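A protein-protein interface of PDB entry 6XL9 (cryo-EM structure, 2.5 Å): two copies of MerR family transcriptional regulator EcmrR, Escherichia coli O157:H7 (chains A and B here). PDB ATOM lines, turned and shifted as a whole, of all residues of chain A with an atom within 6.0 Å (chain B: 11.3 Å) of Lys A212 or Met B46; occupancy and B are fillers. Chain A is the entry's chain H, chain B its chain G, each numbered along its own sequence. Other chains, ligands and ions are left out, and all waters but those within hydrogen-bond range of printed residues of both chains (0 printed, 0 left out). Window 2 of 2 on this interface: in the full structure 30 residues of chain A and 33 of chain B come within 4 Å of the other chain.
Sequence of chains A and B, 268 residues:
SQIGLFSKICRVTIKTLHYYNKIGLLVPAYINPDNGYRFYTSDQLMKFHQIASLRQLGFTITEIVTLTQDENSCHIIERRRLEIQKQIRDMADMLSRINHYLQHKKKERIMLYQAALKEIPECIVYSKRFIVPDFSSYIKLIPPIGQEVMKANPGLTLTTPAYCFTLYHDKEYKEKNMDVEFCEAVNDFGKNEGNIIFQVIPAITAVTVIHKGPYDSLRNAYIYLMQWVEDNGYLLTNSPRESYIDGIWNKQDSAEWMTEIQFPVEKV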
ATOM      1  N   LEU A 112     -14.183   8.809  11.973  1.00  0.00           N
ATOM      2  CA  LEU A 112     -13.383   9.282  10.855  1.00  0.00           C
ATOM      3  C   LEU A 112     -12.720  10.619  11.167  1.00  0.00           C
ATOM      4  O   LEU A 112     -11.523  10.790  10.916  1.00  0.00           O
ATOM      5  CB  LEU A 112     -14.276   9.389   9.616  1.00  0.00           C
ATOM      6  CG  LEU A 112     -13.780   9.486   8.166  1.00  0.00           C
ATOM      7  CD1 LEU A 112     -14.985   9.504   7.260  1.00  0.00           C
ATOM      8  CD2 LEU A 112     -12.915  10.700   7.873  1.00  0.00           C
ATOM      9  N   GLN A 114     -11.263  13.652  13.395  1.00  0.00           N
ATOM     10  CA  GLN A 114     -10.623  13.932  14.676  1.00  0.00           C
ATOM     11  C   GLN A 114     -10.201  15.393  14.680  1.00  0.00           C
ATOM     12  O   GLN A 114      -9.275  15.767  13.956  1.00  0.00           O
ATOM     13  CB  GLN A 114      -9.452  12.975  14.903  1.00  0.00           C
ATOM     14  CG  GLN A 114      -9.888  11.524  14.741  1.00  0.00           C
ATOM     15  CD  GLN A 114      -8.765  10.587  14.386  1.00  0.00           C
ATOM     16  OE1 GLN A 114      -8.179   9.948  15.259  1.00  0.00           O
ATOM     17  NE2 GLN A 114      -8.474  10.474  13.098  1.00  0.00           N
ATOM     18  N   ILE A 210      -9.161  16.732   8.998  1.00  0.00           N
ATOM     19  CA  ILE A 210      -8.620  16.258   7.729  1.00  0.00           C
ATOM     20  C   ILE A 210      -9.582  15.248   7.120  1.00  0.00           C
ATOM     21  O   ILE A 210      -9.993  14.289   7.783  1.00  0.00           O
ATOM     22  CB  ILE A 210      -7.204  15.671   7.882  1.00  0.00           C
ATOM     23  CG1 ILE A 210      -7.164  14.546   8.922  1.00  0.00           C
ATOM     24  CG2 ILE A 210      -6.200  16.770   8.197  1.00  0.00           C
ATOM     25  CD1 ILE A 210      -5.765  14.080   9.265  1.00  0.00           C
ATOM     26  N   HIS A 211      -9.967  15.486   5.869  1.00  0.00           N
ATOM     27  CA  HIS A 211     -10.799  14.576   5.100  1.00  0.00           C
ATOM     28  C   HIS A 211      -9.939  13.847   4.077  1.00  0.00           C
ATOM     29  O   HIS A 211      -9.031  14.436   3.475  1.00  0.00           O
ATOM     30  CB  HIS A 211     -11.931  15.329   4.397  1.00  0.00           C
ATOM     31  CG  HIS A 211     -12.816  14.456   3.565  1.00  0.00           C
ATOM     32  ND1 HIS A 211     -13.698  13.551   4.112  1.00  0.00           N
ATOM     33  CD2 HIS A 211     -12.958  14.357   2.223  1.00  0.00           C
ATOM     34  CE1 HIS A 211     -14.343  12.928   3.141  1.00  0.00           C
ATOM     35  NE2 HIS A 211     -13.912  13.398   1.986  1.00  0.00           N
ATOM     36  N   LYS A 212     -10.252  12.570   3.869  1.00  0.00           N
ATOM     37  CA  LYS A 212      -9.477  11.694   3.001  1.00  0.00           C
ATOM     38  C   LYS A 212     -10.416  10.914   2.100  1.00  0.00           C
ATOM     39  O   LYS A 212     -11.286  10.188   2.588  1.00  0.00           O
ATOM     40  CB  LYS A 212      -8.615  10.728   3.812  1.00  0.00           C
ATOM     41  CG  LYS A 212      -7.594   9.999   2.970  1.00  0.00           C
ATOM     42  CD  LYS A 212      -7.042   8.788   3.681  1.00  0.00           C
ATOM     43  CE  LYS A 212      -6.155   7.993   2.749  1.00  0.00           C
ATOM     44  NZ  LYS A 212      -4.933   8.770   2.399  1.00  0.00           N
ATOM     45  N   GLY A 213     -10.242  11.063   0.792  1.00  0.00           N
ATOM     46  CA  GLY A 213     -11.036  10.332  -0.161  1.00  0.00           C
ATOM     47  C   GLY A 213     -11.636  11.192  -1.248  1.00  0.00           C
ATOM     48  O   GLY A 213     -11.087  12.230  -1.633  1.00  0.00           O
ATOM     49  N   PRO A 214     -12.783  10.768  -1.770  1.00  0.00           N
ATOM     50  CA  PRO A 214     -13.428  11.516  -2.854  1.00  0.00           C
ATOM     51  C   PRO A 214     -14.072  12.805  -2.371  1.00  0.00           C
ATOM     52  O   PRO A 214     -14.351  12.996  -1.186  1.00  0.00           O
ATOM     53  CB  PRO A 214     -14.487  10.540  -3.373  1.00  0.00           C
ATOM     54  CG  PRO A 214     -14.796   9.677  -2.203  1.00  0.00           C
ATOM     55  CD  PRO A 214     -13.508   9.528  -1.447  1.00  0.00           C
ATOM     56  N   ALA A 255      -9.262   8.272  -5.010  1.00  0.00           N
ATOM     57  CA  ALA A 255      -9.681   7.821  -3.693  1.00  0.00           C
ATOM     58  C   ALA A 255      -8.586   7.968  -2.654  1.00  0.00           C
ATOM     59  O   ALA A 255      -8.752   7.497  -1.526  1.00  0.00           O
ATOM     60  CB  ALA A 255     -10.138   6.361  -3.762  1.00  0.00           C
ATOM     61  N   GLU A 256      -7.486   8.632  -3.003  1.00  0.00           N
ATOM     62  CA  GLU A 256      -6.395   8.894  -2.075  1.00  0.00           C
ATOM     63  C   GLU A 256      -6.091  10.378  -1.945  1.00  0.00           C
ATOM     64  O   GLU A 256      -5.048  10.735  -1.390  1.00  0.00           O
ATOM     65  CB  GLU A 256      -5.136   8.133  -2.486  1.00  0.00           C
ATOM     66  CG  GLU A 256      -5.349   6.638  -2.574  1.00  0.00           C
ATOM     67  CD  GLU A 256      -5.927   6.066  -1.295  1.00  0.00           C
ATOM     68  OE1 GLU A 256      -6.888   5.275  -1.378  1.00  0.00           O
ATOM     69  OE2 GLU A 256      -5.428   6.414  -0.203  1.00  0.00           O
ATOM     70  N   TRP A 257      -6.965  11.251  -2.432  1.00  0.00           N
ATOM     71  CA  TRP A 257      -6.727  12.671  -2.261  1.00  0.00           C
ATOM     72  C   TRP A 257      -7.107  13.055  -0.846  1.00  0.00           C
ATOM     73  O   TRP A 257      -8.064  12.528  -0.277  1.00  0.00           O
ATOM     74  CB  TRP A 257      -7.573  13.487  -3.234  1.00  0.00           C
ATOM     75  CG  TRP A 257      -7.324  13.248  -4.683  1.00  0.00           C
ATOM     76  CD1 TRP A 257      -6.352  12.471  -5.245  1.00  0.00           C
ATOM     77  CD2 TRP A 257      -8.100  13.763  -5.761  1.00  0.00           C
ATOM     78  NE1 TRP A 257      -6.469  12.489  -6.614  1.00  0.00           N
ATOM     79  CE2 TRP A 257      -7.537  13.278  -6.953  1.00  0.00           C
ATOM     80  CE3 TRP A 257      -9.217  14.599  -5.834  1.00  0.00           C
ATOM     81  CZ2 TRP A 257      -8.057  13.598  -8.200  1.00  0.00           C
ATOM     82  CZ3 TRP A 257      -9.726  14.919  -7.072  1.00  0.00           C
ATOM     83  CH2 TRP A 257      -9.146  14.421  -8.239  1.00  0.00           C
ATOM     84  N   MET A 258      -6.345  13.977  -0.277  1.00  0.00           N
ATOM     85  CA  MET A 258      -6.527  14.370   1.109  1.00  0.00           C
ATOM     86  C   MET A 258      -6.499  15.887   1.196  1.00  0.00           C
ATOM     87  O   MET A 258      -5.670  16.538   0.549  1.00  0.00           O
ATOM     88  CB  MET A 258      -5.533  13.655   2.040  1.00  0.00           C
ATOM     89  CG  MET A 258      -4.073  13.860   1.808  1.00  0.00           C
ATOM     90  SD  MET A 258      -3.109  12.852   2.957  1.00  0.00           S
ATOM     91  CE  MET A 258      -3.500  13.593   4.539  1.00  0.00           C
ATOM     92  N   THR A 259      -7.472  16.445   1.913  1.00  0.00           N
ATOM     93  CA  THR A 259      -7.577  17.883   2.106  1.00  0.00           C
ATOM     94  C   THR A 259      -7.964  18.135   3.552  1.00  0.00           C
ATOM     95  O   THR A 259      -8.363  17.221   4.270  1.00  0.00           O
ATOM     96  CB  THR A 259      -8.592  18.533   1.153  1.00  0.00           C
ATOM     97  OG1 THR A 259      -8.613  19.951   1.367  1.00  0.00           O
ATOM     98  CG2 THR A 259      -9.983  17.971   1.388  1.00  0.00           C
ATOM     99  N   PHE B   6       9.350  18.397   6.668  1.00  0.00           N
ATOM    100  CA  PHE B   6       8.231  17.794   7.377  1.00  0.00           C
ATOM    101  C   PHE B   6       8.031  18.415   8.751  1.00  0.00           C
ATOM    102  O   PHE B   6       6.907  18.451   9.256  1.00  0.00           O
ATOM    103  CB  PHE B   6       8.454  16.296   7.499  1.00  0.00           C
ATOM    104  CG  PHE B   6       7.263  15.556   7.985  1.00  0.00           C
ATOM    105  CD1 PHE B   6       6.267  15.181   7.110  1.00  0.00           C
ATOM    106  CD2 PHE B   6       7.131  15.237   9.318  1.00  0.00           C
ATOM    107  CE1 PHE B   6       5.162  14.495   7.557  1.00  0.00           C
ATOM    108  CE2 PHE B   6       6.028  14.552   9.769  1.00  0.00           C
ATOM    109  CZ  PHE B   6       5.042  14.182   8.889  1.00  0.00           C
ATOM    110  N   ILE B   9       5.923  21.401   7.935  1.00  0.00           N
ATOM    111  CA  ILE B   9       4.554  21.068   7.562  1.00  0.00           C
ATOM    112  C   ILE B   9       3.703  20.821   8.804  1.00  0.00           C
ATOM    113  O   ILE B   9       2.541  21.239   8.868  1.00  0.00           O
ATOM    114  CB  ILE B   9       4.557  19.863   6.608  1.00  0.00           C
ATOM    115  CG1 ILE B   9       5.013  20.304   5.217  1.00  0.00           C
ATOM    116  CG2 ILE B   9       3.197  19.207   6.547  1.00  0.00           C
ATOM    117  CD1 ILE B   9       5.242  19.167   4.263  1.00  0.00           C
ATOM    118  N   CYS B  10       4.275  20.180   9.824  1.00  0.00           N
ATOM    119  CA  CYS B  10       3.550  19.819  11.035  1.00  0.00           C
ATOM    120  C   CYS B  10       3.702  20.831  12.159  1.00  0.00           C
ATOM    121  O   CYS B  10       2.982  20.729  13.156  1.00  0.00           O
ATOM    122  CB  CYS B  10       4.014  18.451  11.538  1.00  0.00           C
ATOM    123  SG  CYS B  10       3.751  17.105  10.384  1.00  0.00           S
ATOM    124  N   LEU B  17      10.361  14.519  16.753  1.00  0.00           N
ATOM    125  CA  LEU B  17      10.266  13.440  15.775  1.00  0.00           C
ATOM    126  C   LEU B  17      11.257  12.323  16.081  1.00  0.00           C
ATOM    127  O   LEU B  17      10.928  11.137  15.944  1.00  0.00           O
ATOM    128  CB  LEU B  17      10.487  13.988  14.367  1.00  0.00           C
ATOM    129  CG  LEU B  17       9.449  14.965  13.811  1.00  0.00           C
ATOM    130  CD1 LEU B  17       9.863  15.451  12.442  1.00  0.00           C
ATOM    131  CD2 LEU B  17       8.078  14.333  13.750  1.00  0.00           C
ATOM    132  N   LEU B  25       6.269   5.289  18.042  1.00  0.00           N
ATOM    133  CA  LEU B  25       4.957   5.887  17.858  1.00  0.00           C
ATOM    134  C   LEU B  25       4.723   6.337  16.426  1.00  0.00           C
ATOM    135  O   LEU B  25       3.653   6.085  15.864  1.00  0.00           O
ATOM    136  CB  LEU B  25       4.809   7.079  18.800  1.00  0.00           C
ATOM    137  CG  LEU B  25       3.442   7.738  18.893  1.00  0.00           C
ATOM    138  CD1 LEU B  25       2.372   6.703  19.117  1.00  0.00           C
ATOM    139  CD2 LEU B  25       3.443   8.767  20.003  1.00  0.00           C
ATOM    140  N   LEU B  26       5.711   6.992  15.826  1.00  0.00           N
ATOM    141  CA  LEU B  26       5.643   7.476  14.452  1.00  0.00           C
ATOM    142  C   LEU B  26       6.929   7.078  13.749  1.00  0.00           C
ATOM    143  O   LEU B  26       7.977   7.684  13.984  1.00  0.00           O
ATOM    144  CB  LEU B  26       5.459   8.992  14.422  1.00  0.00           C
ATOM    145  CG  LEU B  26       5.038   9.659  13.119  1.00  0.00           C
ATOM    146  CD1 LEU B  26       3.601   9.334  12.799  1.00  0.00           C
ATOM    147  CD2 LEU B  26       5.225  11.156  13.241  1.00  0.00           C
ATOM    148  N   VAL B  27       6.851   6.090  12.876  1.00  0.00           N
ATOM    149  CA  VAL B  27       8.023   5.531  12.209  1.00  0.00           C
ATOM    150  C   VAL B  27       8.062   6.097  10.795  1.00  0.00           C
ATOM    151  O   VAL B  27       7.026   6.104  10.120  1.00  0.00           O
ATOM    152  CB  VAL B  27       7.970   3.997  12.184  1.00  0.00           C
ATOM    153  CG1 VAL B  27       9.075   3.433  11.319  1.00  0.00           C
ATOM    154  CG2 VAL B  27       8.054   3.457  13.597  1.00  0.00           C
ATOM    155  N   TYR B  40       9.615  11.237   4.987  1.00  0.00           N
ATOM    156  CA  TYR B  40       8.229  11.128   5.413  1.00  0.00           C
ATOM    157  C   TYR B  40       7.301  11.349   4.223  1.00  0.00           C
ATOM    158  O   TYR B  40       7.710  11.826   3.163  1.00  0.00           O
ATOM    159  CB  TYR B  40       7.917  12.142   6.518  1.00  0.00           C
ATOM    160  CG  TYR B  40       8.538  11.805   7.848  1.00  0.00           C
ATOM    161  CD1 TYR B  40       7.944  10.894   8.702  1.00  0.00           C
ATOM    162  CD2 TYR B  40       9.729  12.388   8.243  1.00  0.00           C
ATOM    163  CE1 TYR B  40       8.514  10.579   9.911  1.00  0.00           C
ATOM    164  CE2 TYR B  40      10.305  12.080   9.454  1.00  0.00           C
ATOM    165  CZ  TYR B  40       9.693  11.173  10.281  1.00  0.00           C
ATOM    166  OH  TYR B  40      10.257  10.858  11.489  1.00  0.00           O
ATOM    167  N   THR B  41       6.029  11.006   4.421  1.00  0.00           N
ATOM    168  CA  THR B  41       4.998  11.082   3.393  1.00  0.00           C
ATOM    169  C   THR B  41       3.746  11.691   4.007  1.00  0.00           C
ATOM    170  O   THR B  41       3.724  12.060   5.183  1.00  0.00           O
ATOM    171  CB  THR B  41       4.681   9.707   2.793  1.00  0.00           C
ATOM    172  OG1 THR B  41       4.340   8.794   3.842  1.00  0.00           O
ATOM    173  CG2 THR B  41       5.863   9.167   2.012  1.00  0.00           C
ATOM    174  N   SER B  42       2.694  11.812   3.196  1.00  0.00           N
ATOM    175  CA  SER B  42       1.491  12.515   3.637  1.00  0.00           C
ATOM    176  C   SER B  42       0.746  11.735   4.716  1.00  0.00           C
ATOM    177  O   SER B  42       0.175  12.331   5.643  1.00  0.00           O
ATOM    178  CB  SER B  42       0.584  12.795   2.446  1.00  0.00           C
ATOM    179  OG  SER B  42       1.232  13.652   1.522  1.00  0.00           O
ATOM    180  N   ASP B  43       0.723  10.404   4.611  1.00  0.00           N
ATOM    181  CA  ASP B  43       0.033   9.611   5.621  1.00  0.00           C
ATOM    182  C   ASP B  43       0.695   9.753   6.986  1.00  0.00           C
ATOM    183  O   ASP B  43       0.036   9.597   8.021  1.00  0.00           O
ATOM    184  CB  ASP B  43      -0.030   8.149   5.192  1.00  0.00           C
ATOM    185  CG  ASP B  43       1.326   7.582   4.855  1.00  0.00           C
ATOM    186  OD1 ASP B  43       2.309   8.349   4.853  1.00  0.00           O
ATOM    187  OD2 ASP B  43       1.412   6.366   4.588  1.00  0.00           O
ATOM    188  N   GLN B  44       1.984  10.077   7.014  1.00  0.00           N
ATOM    189  CA  GLN B  44       2.606  10.421   8.284  1.00  0.00           C
ATOM    190  C   GLN B  44       1.941  11.651   8.882  1.00  0.00           C
ATOM    191  O   GLN B  44       1.748  11.726  10.096  1.00  0.00           O
ATOM    192  CB  GLN B  44       4.107  10.634   8.110  1.00  0.00           C
ATOM    193  CG  GLN B  44       4.760   9.652   7.165  1.00  0.00           C
ATOM    194  CD  GLN B  44       4.638   8.221   7.636  1.00  0.00           C
ATOM    195  OE1 GLN B  44       4.021   7.391   6.977  1.00  0.00           O
ATOM    196  NE2 GLN B  44       5.221   7.927   8.789  1.00  0.00           N
ATOM    197  N   LEU B  45       1.589  12.632   8.045  1.00  0.00           N
ATOM    198  CA  LEU B  45       0.878  13.797   8.560  1.00  0.00           C
ATOM    199  C   LEU B  45      -0.545  13.457   8.993  1.00  0.00           C
ATOM    200  O   LEU B  45      -1.021  13.968  10.018  1.00  0.00           O
ATOM    201  CB  LEU B  45       0.853  14.898   7.503  1.00  0.00           C
ATOM    202  CG  LEU B  45      -0.014  16.133   7.771  1.00  0.00           C
ATOM    203  CD1 LEU B  45       0.349  16.814   9.079  1.00  0.00           C
ATOM    204  CD2 LEU B  45       0.078  17.110   6.617  1.00  0.00           C
ATOM    205  N   MET B  46      -1.251  12.614   8.227  1.00  0.00           N
ATOM    206  CA  MET B  46      -2.575  12.171   8.672  1.00  0.00           C
ATOM    207  C   MET B  46      -2.508  11.477  10.030  1.00  0.00           C
ATOM    208  O   MET B  46      -3.437  11.601  10.834  1.00  0.00           O
ATOM    209  CB  MET B  46      -3.289  11.296   7.633  1.00  0.00           C
ATOM    210  CG  MET B  46      -2.939   9.838   7.571  1.00  0.00           C
ATOM    211  SD  MET B  46      -3.926   8.977   6.330  1.00  0.00           S
ATOM    212  CE  MET B  46      -5.520   8.934   7.145  1.00  0.00           C
ATOM    213  N   LYS B  47      -1.413  10.764  10.314  1.00  0.00           N
ATOM    214  CA  LYS B  47      -1.293  10.107  11.612  1.00  0.00           C
ATOM    215  C   LYS B  47      -0.823  11.071  12.693  1.00  0.00           C
ATOM    216  O   LYS B  47      -1.227  10.934  13.854  1.00  0.00           O
ATOM    217  CB  LYS B  47      -0.328   8.925  11.515  1.00  0.00           C
ATOM    218  CG  LYS B  47      -0.123   8.181  12.820  1.00  0.00           C
ATOM    219  CD  LYS B  47       0.127   6.708  12.589  1.00  0.00           C
ATOM    220  CE  LYS B  47       0.211   5.964  13.905  1.00  0.00           C
ATOM    221  NZ  LYS B  47       0.716   4.577  13.731  1.00  0.00           N
ATOM    222  N   PHE B  48       0.040  12.027  12.351  1.00  0.00           N
ATOM    223  CA  PHE B  48       0.464  13.005  13.342  1.00  0.00           C
ATOM    224  C   PHE B  48      -0.713  13.844  13.799  1.00  0.00           C
ATOM    225  O   PHE B  48      -0.769  14.257  14.963  1.00  0.00           O
ATOM    226  CB  PHE B  48       1.563  13.899  12.776  1.00  0.00           C
ATOM    227  CG  PHE B  48       2.078  14.913  13.752  1.00  0.00           C
ATOM    228  CD1 PHE B  48       3.079  14.591  14.641  1.00  0.00           C
ATOM    229  CD2 PHE B  48       1.556  16.192  13.778  1.00  0.00           C
ATOM    230  CE1 PHE B  48       3.547  15.522  15.537  1.00  0.00           C
ATOM    231  CE2 PHE B  48       2.021  17.123  14.671  1.00  0.00           C
ATOM    232  CZ  PHE B  48       3.018  16.789  15.551  1.00  0.00           C
ATOM    233  N   HIS B  49      -1.652  14.122  12.893  1.00  0.00           N
ATOM    234  CA  HIS B  49      -2.869  14.824  13.285  1.00  0.00           C
ATOM    235  C   HIS B  49      -3.636  14.039  14.342  1.00  0.00           C
ATOM    236  O   HIS B  49      -4.117  14.609  15.326  1.00  0.00           O
ATOM    237  CB  HIS B  49      -3.745  15.092  12.069  1.00  0.00           C
ATOM    238  CG  HIS B  49      -4.777  16.145  12.304  1.00  0.00           C
ATOM    239  ND1 HIS B  49      -6.095  15.849  12.576  1.00  0.00           N
ATOM    240  CD2 HIS B  49      -4.682  17.494  12.329  1.00  0.00           C
ATOM    241  CE1 HIS B  49      -6.768  16.972  12.749  1.00  0.00           C
ATOM    242  NE2 HIS B  49      -5.934  17.985  12.605  1.00  0.00           N
ATOM    243  N   GLN B  50      -3.749  12.723  14.158  1.00  0.00           N
ATOM    244  CA  GLN B  50      -4.426  11.887  15.141  1.00  0.00           C
ATOM    245  C   GLN B  50      -3.676  11.876  16.464  1.00  0.00           C
ATOM    246  O   GLN B  50      -4.292  11.910  17.535  1.00  0.00           O
ATOM    247  CB  GLN B  50      -4.549  10.466  14.604  1.00  0.00           C
ATOM    248  CG  GLN B  50      -4.994   9.452  15.628  1.00  0.00           C
ATOM    249  CD  GLN B  50      -5.416   8.151  14.993  1.00  0.00           C
ATOM    250  OE1 GLN B  50      -6.427   7.561  15.369  1.00  0.00           O
ATOM    251  NE2 GLN B  50      -4.640   7.693  14.016  1.00  0.00           N
ATOM    252  N   ILE B  51      -2.345  11.808  16.406  1.00  0.00           N
ATOM    253  CA  ILE B  51      -1.533  11.829  17.622  1.00  0.00           C
ATOM    254  C   ILE B  51      -1.776  13.114  18.404  1.00  0.00           C
ATOM    255  O   ILE B  51      -1.984  13.087  19.621  1.00  0.00           O
ATOM    256  CB  ILE B  51      -0.047  11.636  17.282  1.00  0.00           C
ATOM    257  CG1 ILE B  51       0.231  10.163  16.999  1.00  0.00           C
ATOM    258  CG2 ILE B  51       0.831  12.115  18.419  1.00  0.00           C
ATOM    259  CD1 ILE B  51       1.626   9.895  16.513  1.00  0.00           C
ATOM    260  N   ALA B  52      -1.738  14.260  17.721  1.00  0.00           N
ATOM    261  CA  ALA B  52      -1.970  15.528  18.409  1.00  0.00           C
ATOM    262  C   ALA B  52      -3.398  15.614  18.932  1.00  0.00           C
ATOM    263  O   ALA B  52      -3.638  16.137  20.029  1.00  0.00           O
ATOM    264  CB  ALA B  52      -1.679  16.700  17.476  1.00  0.00           C
ATOM    265  N   SER B  53      -4.356  15.093  18.162  1.00  0.00           N
ATOM    266  CA  SER B  53      -5.743  15.072  18.605  1.00  0.00           C
ATOM    267  C   SER B  53      -5.905  14.274  19.891  1.00  0.00           C
ATOM    268  O   SER B  53      -6.599  14.711  20.811  1.00  0.00           O
ATOM    269  CB  SER B  53      -6.628  14.491  17.504  1.00  0.00           C
ATOM    270  OG  SER B  53      -7.970  14.371  17.936  1.00  0.00           O
ATOM    271  N   LEU B  54      -5.223  13.134  19.996  1.00  0.00           N
ATOM    272  CA  LEU B  54      -5.291  12.330  21.214  1.00  0.00           C
ATOM    273  C   LEU B  54      -4.550  13.005  22.359  1.00  0.00           C
ATOM    274  O   LEU B  54      -5.001  12.965  23.508  1.00  0.00           O
ATOM    275  CB  LEU B  54      -4.728  10.938  20.951  1.00  0.00           C
ATOM    276  CG  LEU B  54      -5.712   9.969  20.297  1.00  0.00           C
ATOM    277  CD1 LEU B  54      -5.110   8.579  20.165  1.00  0.00           C
ATOM    278  CD2 LEU B  54      -7.009   9.924  21.080  1.00  0.00           C
ATOM    279  N   ILE B  64      -1.598   6.571  24.556  1.00  0.00           N
ATOM    280  CA  ILE B  64      -1.804   6.956  23.162  1.00  0.00           C
ATOM    281  C   ILE B  64      -1.362   5.825  22.242  1.00  0.00           C
ATOM    282  O   ILE B  64      -2.038   5.500  21.259  1.00  0.00           O
ATOM    283  CB  ILE B  64      -1.100   8.290  22.852  1.00  0.00           C
ATOM    284  CG1 ILE B  64      -1.882   9.441  23.485  1.00  0.00           C
ATOM    285  CG2 ILE B  64      -1.009   8.517  21.365  1.00  0.00           C
ATOM    286  CD1 ILE B  64      -1.283  10.803  23.261  1.00  0.00           C
ATOM    287  N   THR B  68      -3.868   3.814  19.746  1.00  0.00           N
ATOM    288  CA  THR B  68      -3.766   3.784  18.294  1.00  0.00           C
ATOM    289  C   THR B  68      -3.632   2.359  17.766  1.00  0.00           C
ATOM    290  O   THR B  68      -4.407   1.950  16.893  1.00  0.00           O
ATOM    291  CB  THR B  68      -2.576   4.633  17.841  1.00  0.00           C
ATOM    292  OG1 THR B  68      -2.744   5.979  18.303  1.00  0.00           O
ATOM    293  CG2 THR B  68      -2.474   4.633  16.327  1.00  0.00           C
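The backbone carbonyl oxygen (O) of Gln A114 sits close to a ring nitrogen (ND1) of His B49 (3.5 Å).
The side-chain amide oxygen (OE1) of Gln B50 sits close to the side-chain amide oxygen (OE1) of Gln A114, 3.0 Å away.
No position is printed for both chains.
The side-chain amino group of Lys A212 is in salt-bridge range of the side-chain carboxylate of Glu A256.
Among the printed residues, pairs that only touch across the chains: Ile A210 with His B49, Gln A114 with Ser B53, Met A258 with Ser B42, Ile A210 with Met B46, Lys A212 with Met B46 and Met A258 with Met B46.
Of the 12 printed residues of chain A, 4 touch a printed residue of chain B.
Hydrophobic or aromatic side chains of chain A that line the printed part of chain B: Ile A210 and Met A258.
Hydrophobic or aromatic side chains of chain B within 4 Å of the printed part of chain A: Met B46 and His B49.
Along chain B the printed residues that touch a printed residue of chain A span positions 42 to 53.
Among the printed residues, no Asp or Glu carboxylate lies within 4 Å of a Lys or Arg side-chain nitrogen of the other chain.
Of the printed residues of chain B, Gln A114 touches His B49, Gln B50 and Ser B53.
His A211 touches none of the printed residues of chain B.
Lys A212 touches one residue of chain B.
No residue of chain B comes within 4 Å of Glu A256.
Trp A257 touches none of the printed residues of chain B.
Of the printed residues of chain A, Ser B42 touches Met A258.
Of chain A, only Ile A210 (3.7 Å), Lys A212 (3.8 Å) and Met A258 (3.9 Å) come within 4 Å of Met B46.
Printed residues of chain A within 4 Å of His B49: Gln A114 and Ile A210.
Of the printed residues of chain A, Gln B50 touches Gln A114.
Printed residues of chain A within 4 Å of Ser B53: Gln A114 (3.7 Å).
The nearest residue of chain B that does not touch Lys A212 is Asp B43 (5.7 Å).
The nearest residue of chain A that does not touch Met B46 is Gln A114 (5.6 Å).
The nearest printed residue of chain B that does not touch Gln A114 is Leu B54 (5.6 Å).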
